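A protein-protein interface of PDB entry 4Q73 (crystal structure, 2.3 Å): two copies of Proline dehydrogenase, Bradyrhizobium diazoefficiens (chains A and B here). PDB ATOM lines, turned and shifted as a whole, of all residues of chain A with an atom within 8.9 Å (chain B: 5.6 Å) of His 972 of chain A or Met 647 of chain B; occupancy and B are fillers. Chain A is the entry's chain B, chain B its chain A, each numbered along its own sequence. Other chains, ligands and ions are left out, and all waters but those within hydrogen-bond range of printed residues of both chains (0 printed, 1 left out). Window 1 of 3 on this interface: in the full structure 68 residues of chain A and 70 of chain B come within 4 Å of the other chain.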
ATOM      1  N   TYR A 620      17.542  11.201   8.557  1.00  0.00           N
ATOM      2  CA  TYR A 620      18.180  12.437   8.129  1.00  0.00           C
ATOM      3  C   TYR A 620      17.433  13.082   6.970  1.00  0.00           C
ATOM      4  O   TYR A 620      17.149  14.282   7.007  1.00  0.00           O
ATOM      5  CB  TYR A 620      19.641  12.196   7.743  1.00  0.00           C
ATOM      6  CG  TYR A 620      20.318  13.429   7.165  1.00  0.00           C
ATOM      7  CD1 TYR A 620      20.710  14.487   7.989  1.00  0.00           C
ATOM      8  CD2 TYR A 620      20.563  13.535   5.801  1.00  0.00           C
ATOM      9  CE1 TYR A 620      21.315  15.612   7.466  1.00  0.00           C
ATOM     10  CE2 TYR A 620      21.179  14.653   5.272  1.00  0.00           C
ATOM     11  CZ  TYR A 620      21.551  15.683   6.115  1.00  0.00           C
ATOM     12  OH  TYR A 620      22.148  16.795   5.592  1.00  0.00           O
ATOM     13  N   TYR A 621      17.101  12.288   5.950  1.00  0.00           N
ATOM     14  CA  TYR A 621      16.304  12.805   4.836  1.00  0.00           C
ATOM     15  C   TYR A 621      14.917  13.260   5.295  1.00  0.00           C
ATOM     16  O   TYR A 621      14.372  14.225   4.753  1.00  0.00           O
ATOM     17  CB  TYR A 621      16.192  11.791   3.695  1.00  0.00           C
ATOM     18  CG  TYR A 621      17.512  11.525   2.999  1.00  0.00           C
ATOM     19  CD1 TYR A 621      18.486  12.510   2.918  1.00  0.00           C
ATOM     20  CD2 TYR A 621      17.786  10.279   2.436  1.00  0.00           C
ATOM     21  CE1 TYR A 621      19.708  12.264   2.277  1.00  0.00           C
ATOM     22  CE2 TYR A 621      18.991  10.025   1.805  1.00  0.00           C
ATOM     23  CZ  TYR A 621      19.957  11.017   1.742  1.00  0.00           C
ATOM     24  OH  TYR A 621      21.169  10.764   1.123  1.00  0.00           O
ATOM     25  N   GLN A 624      15.588  16.714   6.877  1.00  0.00           N
ATOM     26  CA  GLN A 624      15.927  17.653   5.809  1.00  0.00           C
ATOM     27  C   GLN A 624      14.709  17.859   4.914  1.00  0.00           C
ATOM     28  O   GLN A 624      14.512  18.931   4.340  1.00  0.00           O
ATOM     29  CB  GLN A 624      17.115  17.150   4.992  1.00  0.00           C
ATOM     30  CG  GLN A 624      18.391  17.066   5.805  1.00  0.00           C
ATOM     31  CD  GLN A 624      18.877  18.433   6.243  1.00  0.00           C
ATOM     32  OE1 GLN A 624      19.090  18.681   7.438  1.00  0.00           O
ATOM     33  NE2 GLN A 624      19.058  19.334   5.277  1.00  0.00           N
ATOM     34  N   LEU A 628      13.034  21.503   3.872  1.00  0.00           N
ATOM     35  CA  LEU A 628      13.018  21.897   2.469  1.00  0.00           C
ATOM     36  C   LEU A 628      11.604  21.905   1.860  1.00  0.00           C
ATOM     37  O   LEU A 628      11.225  22.854   1.174  1.00  0.00           O
ATOM     38  CB  LEU A 628      13.955  20.985   1.670  1.00  0.00           C
ATOM     39  CG  LEU A 628      14.249  21.361   0.217  1.00  0.00           C
ATOM     40  CD1 LEU A 628      14.724  22.800   0.137  1.00  0.00           C
ATOM     41  CD2 LEU A 628      15.299  20.416  -0.373  1.00  0.00           C
ATOM     42  N   MET A 647       9.139  23.773  -3.585  1.00  0.00           N
ATOM     43  CA  MET A 647       9.848  22.692  -4.254  1.00  0.00           C
ATOM     44  C   MET A 647       8.927  21.499  -4.340  1.00  0.00           C
ATOM     45  O   MET A 647       8.448  21.022  -3.316  1.00  0.00           O
ATOM     46  CB  MET A 647      11.096  22.304  -3.467  1.00  0.00           C
ATOM     47  CG  MET A 647      11.874  23.502  -2.989  1.00  0.00           C
ATOM     48  SD  MET A 647      13.206  23.799  -4.132  1.00  0.00           S
ATOM     49  CE  MET A 647      14.222  22.452  -3.618  1.00  0.00           C
ATOM     50  N   ILE A 758      21.915  11.691 -11.122  1.00  0.00           N
ATOM     51  CA  ILE A 758      22.754  11.695  -9.939  1.00  0.00           C
ATOM     52  C   ILE A 758      23.524  10.393  -9.955  1.00  0.00           C
ATOM     53  O   ILE A 758      22.934   9.316  -9.838  1.00  0.00           O
ATOM     54  CB  ILE A 758      21.932  11.833  -8.645  1.00  0.00           C
ATOM     55  CG1 ILE A 758      21.241  13.191  -8.617  1.00  0.00           C
ATOM     56  CG2 ILE A 758      22.833  11.658  -7.410  1.00  0.00           C
ATOM     57  CD1 ILE A 758      19.898  13.177  -7.878  1.00  0.00           C
ATOM     58  N   PRO A 955      28.764  14.165   4.767  1.00  0.00           N
ATOM     59  CA  PRO A 955      28.081  14.094   3.462  1.00  0.00           C
ATOM     60  C   PRO A 955      29.037  13.460   2.477  1.00  0.00           C
ATOM     61  O   PRO A 955      30.144  13.962   2.280  1.00  0.00           O
ATOM     62  CB  PRO A 955      27.859  15.560   3.095  1.00  0.00           C
ATOM     63  CG  PRO A 955      27.757  16.261   4.456  1.00  0.00           C
ATOM     64  CD  PRO A 955      28.717  15.516   5.361  1.00  0.00           C
ATOM     65  N   GLY A 965      27.667  14.603  -7.946  1.00  0.00           N
ATOM     66  CA  GLY A 965      27.048  15.348  -6.862  1.00  0.00           C
ATOM     67  C   GLY A 965      25.537  15.335  -7.092  1.00  0.00           C
ATOM     68  O   GLY A 965      25.064  14.877  -8.135  1.00  0.00           O
ATOM     69  N   PRO A 966      24.765  15.823  -6.116  1.00  0.00           N
ATOM     70  CA  PRO A 966      25.277  16.303  -4.824  1.00  0.00           C
ATOM     71  C   PRO A 966      25.589  15.128  -3.880  1.00  0.00           C
ATOM     72  O   PRO A 966      25.264  13.980  -4.200  1.00  0.00           O
ATOM     73  CB  PRO A 966      24.110  17.140  -4.289  1.00  0.00           C
ATOM     74  CG  PRO A 966      22.885  16.445  -4.869  1.00  0.00           C
ATOM     75  CD  PRO A 966      23.306  15.991  -6.247  1.00  0.00           C
ATOM     76  N   LYS A 967      26.215  15.420  -2.744  1.00  0.00           N
ATOM     77  CA  LYS A 967      26.636  14.388  -1.794  1.00  0.00           C
ATOM     78  C   LYS A 967      25.447  13.754  -1.093  1.00  0.00           C
ATOM     79  O   LYS A 967      24.630  14.462  -0.522  1.00  0.00           O
ATOM     80  CB  LYS A 967      27.559  14.987  -0.715  1.00  0.00           C
ATOM     81  CG  LYS A 967      28.942  15.452  -1.170  1.00  0.00           C
ATOM     82  CD  LYS A 967      29.602  16.193  -0.002  1.00  0.00           C
ATOM     83  CE  LYS A 967      31.123  16.303  -0.136  1.00  0.00           C
ATOM     84  NZ  LYS A 967      31.790  14.992   0.067  1.00  0.00           N
ATOM     85  N   ALA A 968      25.381  12.427  -1.081  1.00  0.00           N
ATOM     86  CA  ALA A 968      24.386  11.731  -0.272  1.00  0.00           C
ATOM     87  C   ALA A 968      24.636  11.984   1.217  1.00  0.00           C
ATOM     88  O   ALA A 968      25.769  12.223   1.639  1.00  0.00           O
ATOM     89  CB  ALA A 968      24.400  10.225  -0.566  1.00  0.00           C
ATOM     90  N   GLY A 969      23.572  11.979   2.008  1.00  0.00           N
ATOM     91  CA  GLY A 969      23.702  12.203   3.434  1.00  0.00           C
ATOM     92  C   GLY A 969      24.119  13.620   3.789  1.00  0.00           C
ATOM     93  O   GLY A 969      24.615  13.848   4.883  1.00  0.00           O
ATOM     94  N   GLY A 970      23.929  14.566   2.867  1.00  0.00           N
ATOM     95  CA  GLY A 970      24.215  15.975   3.122  1.00  0.00           C
ATOM     96  C   GLY A 970      23.055  16.906   2.778  1.00  0.00           C
ATOM     97  O   GLY A 970      22.020  16.472   2.276  1.00  0.00           O
ATOM     98  N   PRO A 971      23.229  18.207   3.031  1.00  0.00           N
ATOM     99  CA  PRO A 971      22.112  19.165   2.931  1.00  0.00           C
ATOM    100  C   PRO A 971      21.846  19.689   1.519  1.00  0.00           C
ATOM    101  O   PRO A 971      20.999  20.569   1.362  1.00  0.00           O
ATOM    102  CB  PRO A 971      22.568  20.322   3.841  1.00  0.00           C
ATOM    103  CG  PRO A 971      24.116  20.285   3.702  1.00  0.00           C
ATOM    104  CD  PRO A 971      24.458  18.815   3.585  1.00  0.00           C
ATOM    105  N   HIS A 972      22.560  19.188   0.517  1.00  0.00           N
ATOM    106  CA  HIS A 972      22.334  19.637  -0.854  1.00  0.00           C
ATOM    107  C   HIS A 972      21.745  18.532  -1.710  1.00  0.00           C
ATOM    108  O   HIS A 972      21.598  18.687  -2.922  1.00  0.00           O
ATOM    109  CB  HIS A 972      23.628  20.141  -1.483  1.00  0.00           C
ATOM    110  CG  HIS A 972      24.200  21.333  -0.786  1.00  0.00           C
ATOM    111  ND1 HIS A 972      25.041  21.224   0.301  1.00  0.00           N
ATOM    112  CD2 HIS A 972      24.031  22.658  -1.002  1.00  0.00           C
ATOM    113  CE1 HIS A 972      25.377  22.434   0.718  1.00  0.00           C
ATOM    114  NE2 HIS A 972      24.780  23.319  -0.059  1.00  0.00           N
ATOM    115  N   TYR A 973      21.405  17.420  -1.068  1.00  0.00           N
ATOM    116  CA  TYR A 973      20.961  16.217  -1.775  1.00  0.00           C
ATOM    117  C   TYR A 973      19.494  16.265  -2.223  1.00  0.00           C
ATOM    118  O   TYR A 973      19.208  16.092  -3.399  1.00  0.00           O
ATOM    119  CB  TYR A 973      21.189  15.001  -0.886  1.00  0.00           C
ATOM    120  CG  TYR A 973      21.194  13.661  -1.590  1.00  0.00           C
ATOM    121  CD1 TYR A 973      22.153  13.367  -2.544  1.00  0.00           C
ATOM    122  CD2 TYR A 973      20.280  12.664  -1.251  1.00  0.00           C
ATOM    123  CE1 TYR A 973      22.193  12.134  -3.165  1.00  0.00           C
ATOM    124  CE2 TYR A 973      20.315  11.421  -1.865  1.00  0.00           C
ATOM    125  CZ  TYR A 973      21.282  11.163  -2.821  1.00  0.00           C
ATOM    126  OH  TYR A 973      21.346   9.939  -3.449  1.00  0.00           O
ATOM    127  N   LEU A 974      18.580  16.499  -1.283  1.00  0.00           N
ATOM    128  CA  LEU A 974      17.134  16.451  -1.554  1.00  0.00           C
ATOM    129  C   LEU A 974      16.679  17.413  -2.642  1.00  0.00           C
ATOM    130  O   LEU A 974      15.844  17.061  -3.478  1.00  0.00           O
ATOM    131  CB  LEU A 974      16.334  16.728  -0.282  1.00  0.00           C
ATOM    132  CG  LEU A 974      16.382  15.629   0.781  1.00  0.00           C
ATOM    133  CD1 LEU A 974      15.396  15.923   1.909  1.00  0.00           C
ATOM    134  CD2 LEU A 974      16.114  14.255   0.163  1.00  0.00           C
ATOM    135  N   ALA A 975      17.236  18.619  -2.642  1.00  0.00           N
ATOM    136  CA  ALA A 975      16.866  19.630  -3.637  1.00  0.00           C
ATOM    137  C   ALA A 975      17.001  19.110  -5.068  1.00  0.00           C
ATOM    138  O   ALA A 975      16.214  19.468  -5.953  1.00  0.00           O
ATOM    139  CB  ALA A 975      17.708  20.892  -3.454  1.00  0.00           C
ATOM    140  N   ARG A 976      17.994  18.256  -5.291  1.00  0.00           N
ATOM    141  CA  ARG A 976      18.269  17.801  -6.644  1.00  0.00           C
ATOM    142  C   ARG A 976      17.144  16.915  -7.156  1.00  0.00           C
ATOM    143  O   ARG A 976      16.950  16.794  -8.355  1.00  0.00           O
ATOM    144  CB  ARG A 976      19.594  17.062  -6.700  1.00  0.00           C
ATOM    145  CG  ARG A 976      20.045  16.808  -8.099  1.00  0.00           C
ATOM    146  CD  ARG A 976      20.665  18.051  -8.711  1.00  0.00           C
ATOM    147  NE  ARG A 976      21.191  17.679 -10.019  1.00  0.00           N
ATOM    148  CZ  ARG A 976      20.571  17.932 -11.167  1.00  0.00           C
ATOM    149  NH1 ARG A 976      19.420  18.597 -11.165  1.00  0.00           N
ATOM    150  NH2 ARG A 976      21.107  17.528 -12.311  1.00  0.00           N
ATOM    151  N   PHE A 977      16.404  16.307  -6.236  1.00  0.00           N
ATOM    152  CA  PHE A 977      15.274  15.457  -6.579  1.00  0.00           C
ATOM    153  C   PHE A 977      13.981  16.238  -6.773  1.00  0.00           C
ATOM    154  O   PHE A 977      12.920  15.647  -7.006  1.00  0.00           O
ATOM    155  CB  PHE A 977      15.060  14.413  -5.495  1.00  0.00           C
ATOM    156  CG  PHE A 977      16.140  13.393  -5.432  1.00  0.00           C
ATOM    157  CD1 PHE A 977      17.333  13.676  -4.781  1.00  0.00           C
ATOM    158  CD2 PHE A 977      15.973  12.149  -6.015  1.00  0.00           C
ATOM    159  CE1 PHE A 977      18.361  12.731  -4.713  1.00  0.00           C
ATOM    160  CE2 PHE A 977      16.995  11.193  -5.946  1.00  0.00           C
ATOM    161  CZ  PHE A 977      18.188  11.490  -5.296  1.00  0.00           C
ATOM    162  N   ALA A 978      14.062  17.561  -6.684  1.00  0.00           N
ATOM    163  CA  ALA A 978      12.855  18.376  -6.763  1.00  0.00           C
ATOM    164  C   ALA A 978      12.953  19.416  -7.865  1.00  0.00           C
ATOM    165  O   ALA A 978      14.001  19.618  -8.470  1.00  0.00           O
ATOM    166  CB  ALA A 978      12.560  19.062  -5.398  1.00  0.00           C
ATOM    167  N   LEU B 628      26.816  31.455   0.799  1.00  0.00           N
ATOM    168  CA  LEU B 628      27.090  30.074   0.415  1.00  0.00           C
ATOM    169  C   LEU B 628      28.593  29.727   0.454  1.00  0.00           C
ATOM    170  O   LEU B 628      28.964  28.648   0.898  1.00  0.00           O
ATOM    171  CB  LEU B 628      26.499  29.797  -0.965  1.00  0.00           C
ATOM    172  CG  LEU B 628      26.514  28.330  -1.393  1.00  0.00           C
ATOM    173  CD1 LEU B 628      25.850  27.487  -0.318  1.00  0.00           C
ATOM    174  CD2 LEU B 628      25.825  28.132  -2.750  1.00  0.00           C
ATOM    175  N   PHE B 629      29.452  30.629  -0.015  1.00  0.00           N
ATOM    176  CA  PHE B 629      30.881  30.324  -0.111  1.00  0.00           C
ATOM    177  C   PHE B 629      31.773  31.091   0.876  1.00  0.00           C
ATOM    178  O   PHE B 629      32.999  30.947   0.856  1.00  0.00           O
ATOM    179  CB  PHE B 629      31.381  30.580  -1.536  1.00  0.00           C
ATOM    180  CG  PHE B 629      30.473  30.043  -2.604  1.00  0.00           C
ATOM    181  CD1 PHE B 629      29.775  30.908  -3.429  1.00  0.00           C
ATOM    182  CD2 PHE B 629      30.283  28.680  -2.756  1.00  0.00           C
ATOM    183  CE1 PHE B 629      28.921  30.433  -4.403  1.00  0.00           C
ATOM    184  CE2 PHE B 629      29.423  28.185  -3.744  1.00  0.00           C
ATOM    185  CZ  PHE B 629      28.738  29.069  -4.563  1.00  0.00           C
ATOM    186  N   LEU B 645      31.955  21.186   5.895  1.00  0.00           N
ATOM    187  CA  LEU B 645      31.512  21.088   4.516  1.00  0.00           C
ATOM    188  C   LEU B 645      31.797  22.407   3.799  1.00  0.00           C
ATOM    189  O   LEU B 645      31.446  23.485   4.298  1.00  0.00           O
ATOM    190  CB  LEU B 645      30.011  20.762   4.462  1.00  0.00           C
ATOM    191  CG  LEU B 645      29.368  20.638   3.069  1.00  0.00           C
ATOM    192  CD1 LEU B 645      29.886  19.409   2.298  1.00  0.00           C
ATOM    193  CD2 LEU B 645      27.835  20.628   3.157  1.00  0.00           C
ATOM    194  N   THR B 646      32.451  22.320   2.643  1.00  0.00           N
ATOM    195  CA  THR B 646      32.726  23.495   1.827  1.00  0.00           C
ATOM    196  C   THR B 646      32.235  23.310   0.389  1.00  0.00           C
ATOM    197  O   THR B 646      31.937  22.201  -0.044  1.00  0.00           O
ATOM    198  CB  THR B 646      34.221  23.812   1.788  1.00  0.00           C
ATOM    199  OG1 THR B 646      34.937  22.619   1.466  1.00  0.00           O
ATOM    200  CG2 THR B 646      34.688  24.323   3.135  1.00  0.00           C
ATOM    201  N   MET B 647      32.172  24.415  -0.344  1.00  0.00           N
ATOM    202  CA  MET B 647      31.783  24.416  -1.734  1.00  0.00           C
ATOM    203  C   MET B 647      32.856  25.146  -2.509  1.00  0.00           C
ATOM    204  O   MET B 647      33.133  26.313  -2.234  1.00  0.00           O
ATOM    205  CB  MET B 647      30.454  25.143  -1.909  1.00  0.00           C
ATOM    206  CG  MET B 647      29.453  24.785  -0.853  1.00  0.00           C
ATOM    207  SD  MET B 647      28.404  23.487  -1.469  1.00  0.00           S
ATOM    208  CE  MET B 647      27.432  24.460  -2.584  1.00  0.00           C
ATOM    209  N   ARG B 648      33.446  24.460  -3.482  1.00  0.00           N
ATOM    210  CA  ARG B 648      34.543  25.010  -4.266  1.00  0.00           C
ATOM    211  C   ARG B 648      34.142  25.101  -5.734  1.00  0.00           C
ATOM    212  O   ARG B 648      33.217  24.414  -6.174  1.00  0.00           O
ATOM    213  CB  ARG B 648      35.775  24.100  -4.156  1.00  0.00           C
ATOM    214  CG  ARG B 648      36.081  23.566  -2.771  1.00  0.00           C
ATOM    215  CD  ARG B 648      37.161  22.487  -2.855  1.00  0.00           C
ATOM    216  NE  ARG B 648      38.382  22.970  -3.500  1.00  0.00           N
ATOM    217  CZ  ARG B 648      39.612  22.860  -2.996  1.00  0.00           C
ATOM    218  NH1 ARG B 648      40.647  23.336  -3.683  1.00  0.00           N
ATOM    219  NH2 ARG B 648      39.818  22.261  -1.823  1.00  0.00           N
ATOM    220  N   GLY B 649      34.855  25.926  -6.496  1.00  0.00           N
ATOM    221  CA  GLY B 649      34.658  25.982  -7.937  1.00  0.00           C
ATOM    222  C   GLY B 649      34.802  24.607  -8.569  1.00  0.00           C
ATOM    223  O   GLY B 649      35.432  23.730  -7.977  1.00  0.00           O
ATOM    224  N   ALA B 676      30.926  31.329  -8.039  1.00  0.00           N
ATOM    225  CA  ALA B 676      31.107  30.018  -7.413  1.00  0.00           C
ATOM    226  C   ALA B 676      32.571  29.595  -7.389  1.00  0.00           C
ATOM    227  O   ALA B 676      32.927  28.590  -6.756  1.00  0.00           O
ATOM    228  CB  ALA B 676      30.276  28.983  -8.110  1.00  0.00           C
ATOM    229  N   ALA B 975      24.793  27.040  -5.998  1.00  0.00           N
ATOM    230  CA  ALA B 975      25.282  25.736  -5.551  1.00  0.00           C
ATOM    231  C   ALA B 975      25.653  24.817  -6.704  1.00  0.00           C
ATOM    232  O   ALA B 975      26.637  24.070  -6.650  1.00  0.00           O
ATOM    233  CB  ALA B 975      24.224  25.062  -4.682  1.00  0.00           C
ATOM    234  N   ALA B 978      29.030  24.748  -8.220  1.00  0.00           N
ATOM    235  CA  ALA B 978      30.087  24.378  -7.284  1.00  0.00           C
ATOM    236  C   ALA B 978      30.070  22.897  -7.006  1.00  0.00           C
ATOM    237  O   ALA B 978      29.134  22.197  -7.397  1.00  0.00           O
ATOM    238  CB  ALA B 978      29.967  25.163  -5.960  1.00  0.00           C
ATOM    239  N   THR B 979      31.117  22.423  -6.335  1.00  0.00           N
ATOM    240  CA  THR B 979      31.141  21.050  -5.881  1.00  0.00           C
ATOM    241  C   THR B 979      31.437  21.055  -4.380  1.00  0.00           C
ATOM    242  O   THR B 979      32.116  21.966  -3.884  1.00  0.00           O
ATOM    243  CB  THR B 979      32.151  20.181  -6.699  1.00  0.00           C
ATOM    244  OG1 THR B 979      31.986  18.801  -6.369  1.00  0.00           O
ATOM    245  CG2 THR B 979      33.589  20.606  -6.442  1.00  0.00           C
ATOM    246  N   GLU B 980      30.909  20.060  -3.669  1.00  0.00           N
ATOM    247  CA  GLU B 980      31.047  19.973  -2.220  1.00  0.00           C
ATOM    248  C   GLU B 980      32.305  19.228  -1.783  1.00  0.00           C
ATOM    249  O   GLU B 980      32.736  18.277  -2.427  1.00  0.00           O
ATOM    250  CB  GLU B 980      29.852  19.237  -1.620  1.00  0.00           C
ATOM    251  CG  GLU B 980      28.491  19.816  -1.960  1.00  0.00           C
ATOM    252  CD  GLU B 980      27.382  18.812  -1.704  1.00  0.00           C
ATOM    253  OE1 GLU B 980      26.968  18.671  -0.528  1.00  0.00           O
ATOM    254  OE2 GLU B 980      26.949  18.142  -2.678  1.00  0.00           O
ATOM    255  N   GLN B 981      32.861  19.641  -0.651  1.00  0.00           N
ATOM    256  CA  GLN B 981      34.009  18.954  -0.066  1.00  0.00           C
ATOM    257  C   GLN B 981      33.873  18.867   1.454  1.00  0.00           C
ATOM    258  O   GLN B 981      33.676  19.875   2.148  1.00  0.00           O
ATOM    259  CB  GLN B 981      35.314  19.638  -0.457  1.00  0.00           C
ATOM    260  CG  GLN B 981      36.544  19.029   0.183  1.00  0.00           C
ATOM    261  CD  GLN B 981      37.823  19.610  -0.384  1.00  0.00           C
ATOM    262  OE1 GLN B 981      38.258  20.701   0.014  1.00  0.00           O
ATOM    263  NE2 GLN B 981      38.417  18.902  -1.345  1.00  0.00           N
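N of Lys 967 of chain A sits at hydrogen-bond distance from OE2 of Glu 980 of chain B, at 2.8 Å.
OE1 of Glu 980 of chain B is in hydrogen-bond range of ND1 of His 972 of chain A, at 3.3 Å.
N of Thr 646 of chain B is in hydrogen-bond range of O of Gln 981 of chain B (2.8 Å).
OE1 of Gln 981 of chain B sits at hydrogen-bond distance from NH2 of Arg 648 of chain B, at 2.9 Å.
O of Pro 955 of chain A lies within hydrogen-bond range of NZ of Lys 967 of chain A (2.9 Å).
Pro 966 of chain A touches Glu 980 of chain B.
Lys 967 of chain A touches Leu 645 of chain B.
Lys 967 of chain A touches Gln 981 of chain B.
Leu 645 of chain B touches Pro 971 of chain A (CD2 to CG, 3.8 Å).
His 972 of chain A touches Leu 645 of chain B (CE1 to CD2, 3.9 Å).
NE2 of His 972 of chain A touches CE of Met 647 of chain B, at 3.8 Å.
Of chain B, only Leu 645 (3.9 Å), Met 647 (3.8 Å) and Glu 980 (3.3 Å) come within 4 Å of His 972 of chain A.
Of the printed residues of chain A, Met 647 of chain B touches His 972 (3.8 Å).
Of the printed residues of chain B, Pro 971 of chain A touches Leu 645.
Of the printed residues of chain A, Glu 980 of chain B touches Pro 966, Lys 967 and His 972.
Tyr 620 of chain A touches none of the printed residues of chain B.
Leu 628 of chain B touches none of the printed residues of chain A.
The nearest residue of chain A that does not touch Met 647 of chain B is Pro 971 of chain A (7.4 Å).
Printed residues of chain A that touch a printed residue of chain B: Pro 966, Lys 967, Pro 971 and His 972.
Hydrophobic or aromatic side chains of chain A that line the printed part of chain B: Pro 966, Pro 971 and His 972.
Hydrophobic or aromatic side chains of chain B that line the printed part of chain A: Leu 645 and Met 647.
Among the printed residues, no Asp or Glu carboxylate lies within 4 Å of a Lys or Arg side-chain nitrogen of the other chain.
Positions printed for both chains: 628, 647, 975 and 978.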
